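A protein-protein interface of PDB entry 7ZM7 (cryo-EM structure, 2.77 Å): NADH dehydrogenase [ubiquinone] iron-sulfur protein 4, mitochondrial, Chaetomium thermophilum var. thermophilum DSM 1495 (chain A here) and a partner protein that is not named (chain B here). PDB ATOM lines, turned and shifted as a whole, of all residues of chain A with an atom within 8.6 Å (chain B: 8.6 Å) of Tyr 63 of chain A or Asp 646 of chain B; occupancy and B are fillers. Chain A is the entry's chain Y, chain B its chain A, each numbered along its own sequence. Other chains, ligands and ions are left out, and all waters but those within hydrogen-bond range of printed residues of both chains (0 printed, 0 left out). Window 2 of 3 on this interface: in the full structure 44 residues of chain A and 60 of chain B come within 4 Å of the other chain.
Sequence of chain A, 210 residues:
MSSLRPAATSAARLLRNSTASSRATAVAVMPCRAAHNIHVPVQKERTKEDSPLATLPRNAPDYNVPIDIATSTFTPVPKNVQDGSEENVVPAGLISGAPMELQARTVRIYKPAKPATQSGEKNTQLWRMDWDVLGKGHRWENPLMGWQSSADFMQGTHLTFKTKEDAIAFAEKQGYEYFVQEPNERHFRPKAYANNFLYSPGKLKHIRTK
O of Arg 58 of chain A sits at hydrogen-bond distance from NE2 of Gln 650 of chain B, 3.4 Å away. The backbone carbonyl oxygen (O) of Ala 649 of chain B lies close to the side-chain amide nitrogen (ND2) of Asn 59 of chain A (3.5 Å).
N of Asp 646 of chain B sits at hydrogen-bond distance from OE1 of Gln 650 of chain B, at 2.8 Å. The backbone NH (N) of Asp 647 of chain B sits at hydrogen-bond distance from the side-chain amide oxygen (OE1) of Gln 650 of chain B (3.3 Å).
Asn 59 of chain A touches Gln 650 of chain B (O to CG, 3.2 Å). Gln 650 of chain B touches Ala 60 of chain A. OD1 of Asp 646 of chain B touches CG of Pro 61 of chain A, at 3.1 Å. Gln 650 of chain B touches Pro 61 of chain A (OE1 to CD, 3.98 Å). Asp 646 of chain B touches Tyr 63 of chain A (OD1 to OH, 3.6 Å). Lys 79 of chain A touches Asp 647 of chain B (CD to OD2, 3.2 Å).
Of chain B, only Asp 646 (3.6 Å) comes within 4 Å of Tyr 63 of chain A. Of chain A, only Pro 61 and Tyr 63 come within 4 Å of Asp 646 of chain B. Of the printed residues of chain B, Asn 59 of chain A touches Ala 649 (3.3 Å) and Gln 650 (3.2 Å). Printed residues of chain B within 4 Å of Ala 60 of chain A: Gln 650 (3.9 Å).
Printed residues of chain A that touch a printed residue of chain B: Arg 58, Asn 59, Ala 60, Pro 61, Tyr 63 and Lys 79. Hydrophobic or aromatic side chains of chain A that line the printed part of chain B: Pro 61 and Tyr 63. Printed residues of chain B that touch a printed residue of chain A: Asp 646, Asp 647, Ala 649 and Gln 650. Hydrophobic or aromatic side chains of chain B that line the printed part of chain A: Ala 649.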
ATOM      1  N   ARG A  58     -17.609 -36.079   2.306  1.00  0.00           N
ATOM      2  CA  ARG A  58     -17.619 -35.682   3.714  1.00  0.00           C
ATOM      3  C   ARG A  58     -17.198 -34.217   3.879  1.00  0.00           C
ATOM      4  O   ARG A  58     -16.101 -33.899   4.342  1.00  0.00           O
ATOM      5  CB  ARG A  58     -16.727 -36.616   4.540  1.00  0.00           C
ATOM      6  CG  ARG A  58     -16.944 -36.520   6.035  1.00  0.00           C
ATOM      7  CD  ARG A  58     -18.389 -36.811   6.388  1.00  0.00           C
ATOM      8  NE  ARG A  58     -18.639 -36.673   7.818  1.00  0.00           N
ATOM      9  CZ  ARG A  58     -19.848 -36.566   8.355  1.00  0.00           C
ATOM     10  NH1 ARG A  58     -20.923 -36.579   7.579  1.00  0.00           N
ATOM     11  NH2 ARG A  58     -19.984 -36.443   9.668  1.00  0.00           N
ATOM     12  N   ASN A  59     -18.095 -33.334   3.435  1.00  0.00           N
ATOM     13  CA  ASN A  59     -17.978 -31.888   3.592  1.00  0.00           C
ATOM     14  C   ASN A  59     -16.875 -31.287   2.737  1.00  0.00           C
ATOM     15  O   ASN A  59     -16.417 -30.175   3.005  1.00  0.00           O
ATOM     16  CB  ASN A  59     -17.759 -31.498   5.057  1.00  0.00           C
ATOM     17  CG  ASN A  59     -19.035 -31.511   5.856  1.00  0.00           C
ATOM     18  OD1 ASN A  59     -20.100 -31.823   5.335  1.00  0.00           O
ATOM     19  ND2 ASN A  59     -18.936 -31.174   7.134  1.00  0.00           N
ATOM     20  N   ALA A  60     -16.426 -31.998   1.729  1.00  0.00           N
ATOM     21  CA  ALA A  60     -15.390 -31.475   0.855  1.00  0.00           C
ATOM     22  C   ALA A  60     -16.001 -30.478  -0.119  1.00  0.00           C
ATOM     23  O   ALA A  60     -16.999 -30.795  -0.770  1.00  0.00           O
ATOM     24  CB  ALA A  60     -14.704 -32.602   0.092  1.00  0.00           C
ATOM     25  N   PRO A  61     -15.448 -29.274  -0.234  1.00  0.00           N
ATOM     26  CA  PRO A  61     -16.004 -28.284  -1.159  1.00  0.00           C
ATOM     27  C   PRO A  61     -15.794 -28.720  -2.601  1.00  0.00           C
ATOM     28  O   PRO A  61     -14.665 -28.933  -3.036  1.00  0.00           O
ATOM     29  CB  PRO A  61     -15.211 -27.014  -0.830  1.00  0.00           C
ATOM     30  CG  PRO A  61     -13.940 -27.502  -0.274  1.00  0.00           C
ATOM     31  CD  PRO A  61     -14.259 -28.763   0.466  1.00  0.00           C
ATOM     32  N   ASP A  62     -16.886 -28.850  -3.344  1.00  0.00           N
ATOM     33  CA  ASP A  62     -16.806 -29.259  -4.741  1.00  0.00           C
ATOM     34  C   ASP A  62     -16.278 -28.086  -5.539  1.00  0.00           C
ATOM     35  O   ASP A  62     -17.046 -27.267  -6.046  1.00  0.00           O
ATOM     36  CB  ASP A  62     -18.160 -29.715  -5.263  1.00  0.00           C
ATOM     37  CG  ASP A  62     -18.044 -30.626  -6.477  1.00  0.00           C
ATOM     38  OD1 ASP A  62     -17.353 -31.663  -6.383  1.00  0.00           O
ATOM     39  OD2 ASP A  62     -18.650 -30.313  -7.524  1.00  0.00           O
ATOM     40  N   TYR A  63     -14.952 -28.023  -5.666  1.00  0.00           N
ATOM     41  CA  TYR A  63     -14.292 -26.947  -6.390  1.00  0.00           C
ATOM     42  C   TYR A  63     -14.587 -26.984  -7.875  1.00  0.00           C
ATOM     43  O   TYR A  63     -14.247 -26.028  -8.577  1.00  0.00           O
ATOM     44  CB  TYR A  63     -12.787 -27.005  -6.175  1.00  0.00           C
ATOM     45  CG  TYR A  63     -12.316 -26.478  -4.850  1.00  0.00           C
ATOM     46  CD1 TYR A  63     -12.450 -25.148  -4.524  1.00  0.00           C
ATOM     47  CD2 TYR A  63     -11.694 -27.310  -3.939  1.00  0.00           C
ATOM     48  CE1 TYR A  63     -12.011 -24.665  -3.319  1.00  0.00           C
ATOM     49  CE2 TYR A  63     -11.245 -26.837  -2.740  1.00  0.00           C
ATOM     50  CZ  TYR A  63     -11.407 -25.513  -2.430  1.00  0.00           C
ATOM     51  OH  TYR A  63     -10.968 -25.047  -1.221  1.00  0.00           O
ATOM     52  N   ASN A  64     -15.203 -28.054  -8.372  1.00  0.00           N
ATOM     53  CA  ASN A  64     -15.494 -28.192  -9.789  1.00  0.00           C
ATOM     54  C   ASN A  64     -16.973 -28.048 -10.106  1.00  0.00           C
ATOM     55  O   ASN A  64     -17.420 -28.532 -11.148  1.00  0.00           O
ATOM     56  CB  ASN A  64     -14.987 -29.535 -10.314  1.00  0.00           C
ATOM     57  CG  ASN A  64     -13.482 -29.617 -10.343  1.00  0.00           C
ATOM     58  OD1 ASN A  64     -12.893 -30.584  -9.867  1.00  0.00           O
ATOM     59  ND2 ASN A  64     -12.846 -28.595 -10.897  1.00  0.00           N
ATOM     60  N   VAL A  65     -17.744 -27.403  -9.243  1.00  0.00           N
ATOM     61  CA  VAL A  65     -19.137 -27.129  -9.570  1.00  0.00           C
ATOM     62  C   VAL A  65     -19.166 -26.253 -10.814  1.00  0.00           C
ATOM     63  O   VAL A  65     -18.315 -25.363 -10.967  1.00  0.00           O
ATOM     64  CB  VAL A  65     -19.869 -26.434  -8.418  1.00  0.00           C
ATOM     65  CG1 VAL A  65     -20.154 -27.401  -7.304  1.00  0.00           C
ATOM     66  CG2 VAL A  65     -19.047 -25.277  -7.923  1.00  0.00           C
ATOM     67  N   PRO A  66     -20.104 -26.463 -11.719  1.00  0.00           N
ATOM     68  CA  PRO A  66     -20.236 -25.553 -12.859  1.00  0.00           C
ATOM     69  C   PRO A  66     -20.892 -24.248 -12.449  1.00  0.00           C
ATOM     70  O   PRO A  66     -22.038 -24.243 -11.996  1.00  0.00           O
ATOM     71  CB  PRO A  66     -21.104 -26.342 -13.844  1.00  0.00           C
ATOM     72  CG  PRO A  66     -21.841 -27.328 -13.014  1.00  0.00           C
ATOM     73  CD  PRO A  66     -21.085 -27.558 -11.744  1.00  0.00           C
ATOM     74  N   ILE A  67     -20.170 -23.137 -12.601  1.00  0.00           N
ATOM     75  CA  ILE A  67     -20.684 -21.829 -12.213  1.00  0.00           C
ATOM     76  C   ILE A  67     -21.803 -21.410 -13.153  1.00  0.00           C
ATOM     77  O   ILE A  67     -22.047 -22.050 -14.182  1.00  0.00           O
ATOM     78  CB  ILE A  67     -19.556 -20.788 -12.229  1.00  0.00           C
ATOM     79  CG1 ILE A  67     -19.007 -20.650 -13.643  1.00  0.00           C
ATOM     80  CG2 ILE A  67     -18.444 -21.189 -11.279  1.00  0.00           C
ATOM     81  CD1 ILE A  67     -18.072 -19.510 -13.815  1.00  0.00           C
ATOM     82  N   PRO A  76     -18.885 -18.180  -2.528  1.00  0.00           N
ATOM     83  CA  PRO A  76     -18.091 -19.242  -1.916  1.00  0.00           C
ATOM     84  C   PRO A  76     -18.203 -20.534  -2.707  1.00  0.00           C
ATOM     85  O   PRO A  76     -19.060 -20.698  -3.577  1.00  0.00           O
ATOM     86  CB  PRO A  76     -18.704 -19.379  -0.527  1.00  0.00           C
ATOM     87  CG  PRO A  76     -19.509 -18.135  -0.345  1.00  0.00           C
ATOM     88  CD  PRO A  76     -20.011 -17.792  -1.673  1.00  0.00           C
ATOM     89  N   VAL A  77     -17.290 -21.452  -2.417  1.00  0.00           N
ATOM     90  CA  VAL A  77     -17.309 -22.755  -3.071  1.00  0.00           C
ATOM     91  C   VAL A  77     -18.307 -23.641  -2.336  1.00  0.00           C
ATOM     92  O   VAL A  77     -18.191 -23.829  -1.117  1.00  0.00           O
ATOM     93  CB  VAL A  77     -15.908 -23.386  -3.119  1.00  0.00           C
ATOM     94  CG1 VAL A  77     -15.985 -24.814  -3.623  1.00  0.00           C
ATOM     95  CG2 VAL A  77     -14.992 -22.575  -4.013  1.00  0.00           C
ATOM     96  N   PRO A  78     -19.305 -24.183  -3.019  1.00  0.00           N
ATOM     97  CA  PRO A  78     -20.282 -25.042  -2.350  1.00  0.00           C
ATOM     98  C   PRO A  78     -19.737 -26.434  -2.080  1.00  0.00           C
ATOM     99  O   PRO A  78     -18.796 -26.902  -2.715  1.00  0.00           O
ATOM    100  CB  PRO A  78     -21.438 -25.092  -3.346  1.00  0.00           C
ATOM    101  CG  PRO A  78     -20.785 -24.903  -4.652  1.00  0.00           C
ATOM    102  CD  PRO A  78     -19.603 -24.022  -4.447  1.00  0.00           C
ATOM    103  N   LYS A  79     -20.351 -27.093  -1.101  1.00  0.00           N
ATOM    104  CA  LYS A  79     -20.093 -28.507  -0.878  1.00  0.00           C
ATOM    105  C   LYS A  79     -21.099 -29.401  -1.584  1.00  0.00           C
ATOM    106  O   LYS A  79     -20.712 -30.398  -2.195  1.00  0.00           O
ATOM    107  CB  LYS A  79     -20.095 -28.825   0.610  1.00  0.00           C
ATOM    108  CG  LYS A  79     -19.353 -27.838   1.454  1.00  0.00           C
ATOM    109  CD  LYS A  79     -19.295 -28.297   2.884  1.00  0.00           C
ATOM    110  CE  LYS A  79     -20.632 -28.803   3.359  1.00  0.00           C
ATOM    111  NZ  LYS A  79     -21.624 -27.702   3.493  1.00  0.00           N
ATOM    112  N   ASN A  80     -22.382 -29.073  -1.527  1.00  0.00           N
ATOM    113  CA  ASN A  80     -23.424 -29.922  -2.086  1.00  0.00           C
ATOM    114  C   ASN A  80     -24.385 -29.076  -2.899  1.00  0.00           C
ATOM    115  O   ASN A  80     -24.851 -28.036  -2.433  1.00  0.00           O
ATOM    116  CB  ASN A  80     -24.188 -30.645  -0.983  1.00  0.00           C
ATOM    117  CG  ASN A  80     -23.291 -31.428  -0.090  1.00  0.00           C
ATOM    118  OD1 ASN A  80     -23.145 -31.119   1.087  1.00  0.00           O
ATOM    119  ND2 ASN A  80     -22.671 -32.455  -0.641  1.00  0.00           N
ATOM    120  N   MET A 100     -26.218 -20.724  -7.978  1.00  0.00           N
ATOM    121  CA  MET A 100     -25.623 -21.765  -7.153  1.00  0.00           C
ATOM    122  C   MET A 100     -25.191 -21.252  -5.789  1.00  0.00           C
ATOM    123  O   MET A 100     -25.137 -22.032  -4.835  1.00  0.00           O
ATOM    124  CB  MET A 100     -24.446 -22.373  -7.921  1.00  0.00           C
ATOM    125  CG  MET A 100     -23.437 -23.162  -7.112  1.00  0.00           C
ATOM    126  SD  MET A 100     -22.047 -22.116  -6.637  1.00  0.00           S
ATOM    127  CE  MET A 100     -21.134 -22.052  -8.170  1.00  0.00           C
ATOM    128  N   TRP B 629      -8.541 -19.369  11.526  1.00  0.00           N
ATOM    129  CA  TRP B 629      -8.264 -20.769  11.220  1.00  0.00           C
ATOM    130  C   TRP B 629      -7.739 -20.942   9.803  1.00  0.00           C
ATOM    131  O   TRP B 629      -6.987 -21.881   9.541  1.00  0.00           O
ATOM    132  CB  TRP B 629      -9.512 -21.635  11.434  1.00  0.00           C
ATOM    133  CG  TRP B 629     -10.530 -21.593  10.324  1.00  0.00           C
ATOM    134  CD1 TRP B 629     -11.642 -20.821  10.278  1.00  0.00           C
ATOM    135  CD2 TRP B 629     -10.526 -22.356   9.109  1.00  0.00           C
ATOM    136  NE1 TRP B 629     -12.330 -21.045   9.122  1.00  0.00           N
ATOM    137  CE2 TRP B 629     -11.664 -21.981   8.381  1.00  0.00           C
ATOM    138  CE3 TRP B 629      -9.669 -23.315   8.568  1.00  0.00           C
ATOM    139  CZ2 TRP B 629     -11.971 -22.530   7.143  1.00  0.00           C
ATOM    140  CZ3 TRP B 629      -9.974 -23.859   7.342  1.00  0.00           C
ATOM    141  CH2 TRP B 629     -11.114 -23.463   6.638  1.00  0.00           C
ATOM    142  N   LYS B 630      -8.107 -20.047   8.882  1.00  0.00           N
ATOM    143  CA  LYS B 630      -7.586 -20.133   7.524  1.00  0.00           C
ATOM    144  C   LYS B 630      -6.134 -19.686   7.413  1.00  0.00           C
ATOM    145  O   LYS B 630      -5.436 -20.117   6.496  1.00  0.00           O
ATOM    146  CB  LYS B 630      -8.448 -19.324   6.563  1.00  0.00           C
ATOM    147  CG  LYS B 630      -9.831 -19.860   6.328  1.00  0.00           C
ATOM    148  CD  LYS B 630     -10.529 -18.980   5.342  1.00  0.00           C
ATOM    149  CE  LYS B 630     -11.921 -19.420   5.050  1.00  0.00           C
ATOM    150  NZ  LYS B 630     -12.527 -18.478   4.071  1.00  0.00           N
ATOM    151  N   ARG B 633      -4.341 -22.809   8.159  1.00  0.00           N
ATOM    152  CA  ARG B 633      -4.488 -23.832   7.134  1.00  0.00           C
ATOM    153  C   ARG B 633      -3.645 -23.522   5.911  1.00  0.00           C
ATOM    154  O   ARG B 633      -3.185 -24.436   5.227  1.00  0.00           O
ATOM    155  CB  ARG B 633      -5.966 -23.973   6.771  1.00  0.00           C
ATOM    156  CG  ARG B 633      -6.255 -24.642   5.454  1.00  0.00           C
ATOM    157  CD  ARG B 633      -6.003 -26.121   5.507  1.00  0.00           C
ATOM    158  NE  ARG B 633      -6.277 -26.762   4.229  1.00  0.00           N
ATOM    159  CZ  ARG B 633      -5.456 -26.732   3.188  1.00  0.00           C
ATOM    160  NH1 ARG B 633      -4.307 -26.089   3.261  1.00  0.00           N
ATOM    161  NH2 ARG B 633      -5.789 -27.347   2.073  1.00  0.00           N
ATOM    162  N   ALA B 634      -3.441 -22.245   5.618  1.00  0.00           N
ATOM    163  CA  ALA B 634      -2.619 -21.846   4.484  1.00  0.00           C
ATOM    164  C   ALA B 634      -1.131 -22.022   4.770  1.00  0.00           C
ATOM    165  O   ALA B 634      -0.386 -22.495   3.909  1.00  0.00           O
ATOM    166  CB  ALA B 634      -2.929 -20.397   4.121  1.00  0.00           C
ATOM    167  N   GLU B 637       0.268 -25.280   3.783  1.00  0.00           N
ATOM    168  CA  GLU B 637       0.808 -25.480   2.443  1.00  0.00           C
ATOM    169  C   GLU B 637       2.242 -24.992   2.341  1.00  0.00           C
ATOM    170  O   GLU B 637       3.082 -25.644   1.715  1.00  0.00           O
ATOM    171  CB  GLU B 637      -0.050 -24.774   1.397  1.00  0.00           C
ATOM    172  CG  GLU B 637      -1.436 -25.323   1.210  1.00  0.00           C
ATOM    173  CD  GLU B 637      -1.403 -26.717   0.623  1.00  0.00           C
ATOM    174  OE1 GLU B 637      -0.469 -27.010  -0.155  1.00  0.00           O
ATOM    175  OE2 GLU B 637      -2.319 -27.514   0.905  1.00  0.00           O
ATOM    176  N   PRO B 642      -0.028 -29.837   4.764  1.00  0.00           N
ATOM    177  CA  PRO B 642      -1.366 -29.241   4.700  1.00  0.00           C
ATOM    178  C   PRO B 642      -2.365 -29.965   5.589  1.00  0.00           C
ATOM    179  O   PRO B 642      -2.570 -31.174   5.468  1.00  0.00           O
ATOM    180  CB  PRO B 642      -1.732 -29.367   3.220  1.00  0.00           C
ATOM    181  CG  PRO B 642      -0.903 -30.506   2.722  1.00  0.00           C
ATOM    182  CD  PRO B 642       0.380 -30.431   3.482  1.00  0.00           C
ATOM    183  N   LEU B 643      -2.984 -29.204   6.489  1.00  0.00           N
ATOM    184  CA  LEU B 643      -4.019 -29.744   7.352  1.00  0.00           C
ATOM    185  C   LEU B 643      -5.223 -30.134   6.506  1.00  0.00           C
ATOM    186  O   LEU B 643      -5.669 -29.343   5.676  1.00  0.00           O
ATOM    187  CB  LEU B 643      -4.425 -28.722   8.404  1.00  0.00           C
ATOM    188  CG  LEU B 643      -3.322 -27.971   9.131  1.00  0.00           C
ATOM    189  CD1 LEU B 643      -3.886 -27.136  10.243  1.00  0.00           C
ATOM    190  CD2 LEU B 643      -2.314 -28.966   9.675  1.00  0.00           C
ATOM    191  N   PRO B 644      -5.786 -31.322   6.718  1.00  0.00           N
ATOM    192  CA  PRO B 644      -6.664 -31.933   5.714  1.00  0.00           C
ATOM    193  C   PRO B 644      -7.868 -31.093   5.329  1.00  0.00           C
ATOM    194  O   PRO B 644      -8.067 -30.764   4.157  1.00  0.00           O
ATOM    195  CB  PRO B 644      -7.101 -33.231   6.397  1.00  0.00           C
ATOM    196  CG  PRO B 644      -6.893 -32.990   7.834  1.00  0.00           C
ATOM    197  CD  PRO B 644      -5.713 -32.127   7.941  1.00  0.00           C
ATOM    198  N   TYR B 645      -8.659 -30.734   6.333  1.00  0.00           N
ATOM    199  CA  TYR B 645      -9.848 -29.920   6.142  1.00  0.00           C
ATOM    200  C   TYR B 645      -9.517 -28.614   5.433  1.00  0.00           C
ATOM    201  O   TYR B 645      -8.501 -27.981   5.704  1.00  0.00           O
ATOM    202  CB  TYR B 645     -10.462 -29.616   7.499  1.00  0.00           C
ATOM    203  CG  TYR B 645      -9.421 -29.387   8.566  1.00  0.00           C
ATOM    204  CD1 TYR B 645      -8.687 -28.222   8.596  1.00  0.00           C
ATOM    205  CD2 TYR B 645      -9.179 -30.337   9.539  1.00  0.00           C
ATOM    206  CE1 TYR B 645      -7.742 -28.012   9.542  1.00  0.00           C
ATOM    207  CE2 TYR B 645      -8.238 -30.128  10.494  1.00  0.00           C
ATOM    208  CZ  TYR B 645      -7.522 -28.960  10.494  1.00  0.00           C
ATOM    209  OH  TYR B 645      -6.572 -28.726  11.450  1.00  0.00           O
ATOM    210  N   ASP B 646     -10.379 -28.210   4.511  1.00  0.00           N
ATOM    211  CA  ASP B 646     -10.235 -26.896   3.900  1.00  0.00           C
ATOM    212  C   ASP B 646     -11.577 -26.198   3.701  1.00  0.00           C
ATOM    213  O   ASP B 646     -11.690 -25.293   2.873  1.00  0.00           O
ATOM    214  CB  ASP B 646      -9.393 -26.995   2.618  1.00  0.00           C
ATOM    215  CG  ASP B 646     -10.137 -27.528   1.430  1.00  0.00           C
ATOM    216  OD1 ASP B 646     -11.374 -27.550   1.403  1.00  0.00           O
ATOM    217  OD2 ASP B 646      -9.445 -27.925   0.483  1.00  0.00           O
ATOM    218  N   ASP B 647     -12.583 -26.613   4.458  1.00  0.00           N
ATOM    219  CA  ASP B 647     -13.826 -25.895   4.667  1.00  0.00           C
ATOM    220  C   ASP B 647     -14.102 -25.944   6.157  1.00  0.00           C
ATOM    221  O   ASP B 647     -13.699 -26.889   6.833  1.00  0.00           O
ATOM    222  CB  ASP B 647     -14.988 -26.519   3.906  1.00  0.00           C
ATOM    223  CG  ASP B 647     -16.025 -25.505   3.497  1.00  0.00           C
ATOM    224  OD1 ASP B 647     -15.650 -24.339   3.249  1.00  0.00           O
ATOM    225  OD2 ASP B 647     -17.215 -25.873   3.401  1.00  0.00           O
ATOM    226  N   VAL B 648     -14.770 -24.916   6.680  1.00  0.00           N
ATOM    227  CA  VAL B 648     -14.936 -24.841   8.128  1.00  0.00           C
ATOM    228  C   VAL B 648     -15.887 -25.921   8.605  1.00  0.00           C
ATOM    229  O   VAL B 648     -15.875 -26.296   9.780  1.00  0.00           O
ATOM    230  CB  VAL B 648     -15.410 -23.438   8.551  1.00  0.00           C
ATOM    231  CG1 VAL B 648     -16.839 -23.196   8.118  1.00  0.00           C
ATOM    232  CG2 VAL B 648     -15.221 -23.223  10.029  1.00  0.00           C
ATOM    233  N   ALA B 649     -16.731 -26.435   7.715  1.00  0.00           N
ATOM    234  CA  ALA B 649     -17.561 -27.572   8.071  1.00  0.00           C
ATOM    235  C   ALA B 649     -16.703 -28.776   8.413  1.00  0.00           C
ATOM    236  O   ALA B 649     -16.952 -29.460   9.410  1.00  0.00           O
ATOM    237  CB  ALA B 649     -18.512 -27.895   6.930  1.00  0.00           C
ATOM    238  N   GLN B 650     -15.663 -29.024   7.616  1.00  0.00           N
ATOM    239  CA  GLN B 650     -14.732 -30.101   7.915  1.00  0.00           C
ATOM    240  C   GLN B 650     -13.994 -29.872   9.221  1.00  0.00           C
ATOM    241  O   GLN B 650     -13.739 -30.826   9.958  1.00  0.00           O
ATOM    242  CB  GLN B 650     -13.728 -30.253   6.797  1.00  0.00           C
ATOM    243  CG  GLN B 650     -14.279 -30.152   5.423  1.00  0.00           C
ATOM    244  CD  GLN B 650     -13.296 -30.648   4.403  1.00  0.00           C
ATOM    245  OE1 GLN B 650     -12.508 -29.882   3.861  1.00  0.00           O
ATOM    246  NE2 GLN B 650     -13.323 -31.943   4.148  1.00  0.00           N
ATOM    247  N   LEU B 651     -13.619 -28.631   9.514  1.00  0.00           N
ATOM    248  CA  LEU B 651     -12.884 -28.377  10.739  1.00  0.00           C
ATOM    249  C   LEU B 651     -13.777 -28.554  11.964  1.00  0.00           C
ATOM    250  O   LEU B 651     -13.275 -28.757  13.071  1.00  0.00           O
ATOM    251  CB  LEU B 651     -12.255 -26.990  10.671  1.00  0.00           C
ATOM    252  CG  LEU B 651     -11.264 -26.505  11.738  1.00  0.00           C
ATOM    253  CD1 LEU B 651     -10.358 -25.491  11.144  1.00  0.00           C
ATOM    254  CD2 LEU B 651     -11.961 -25.892  12.898  1.00  0.00           C
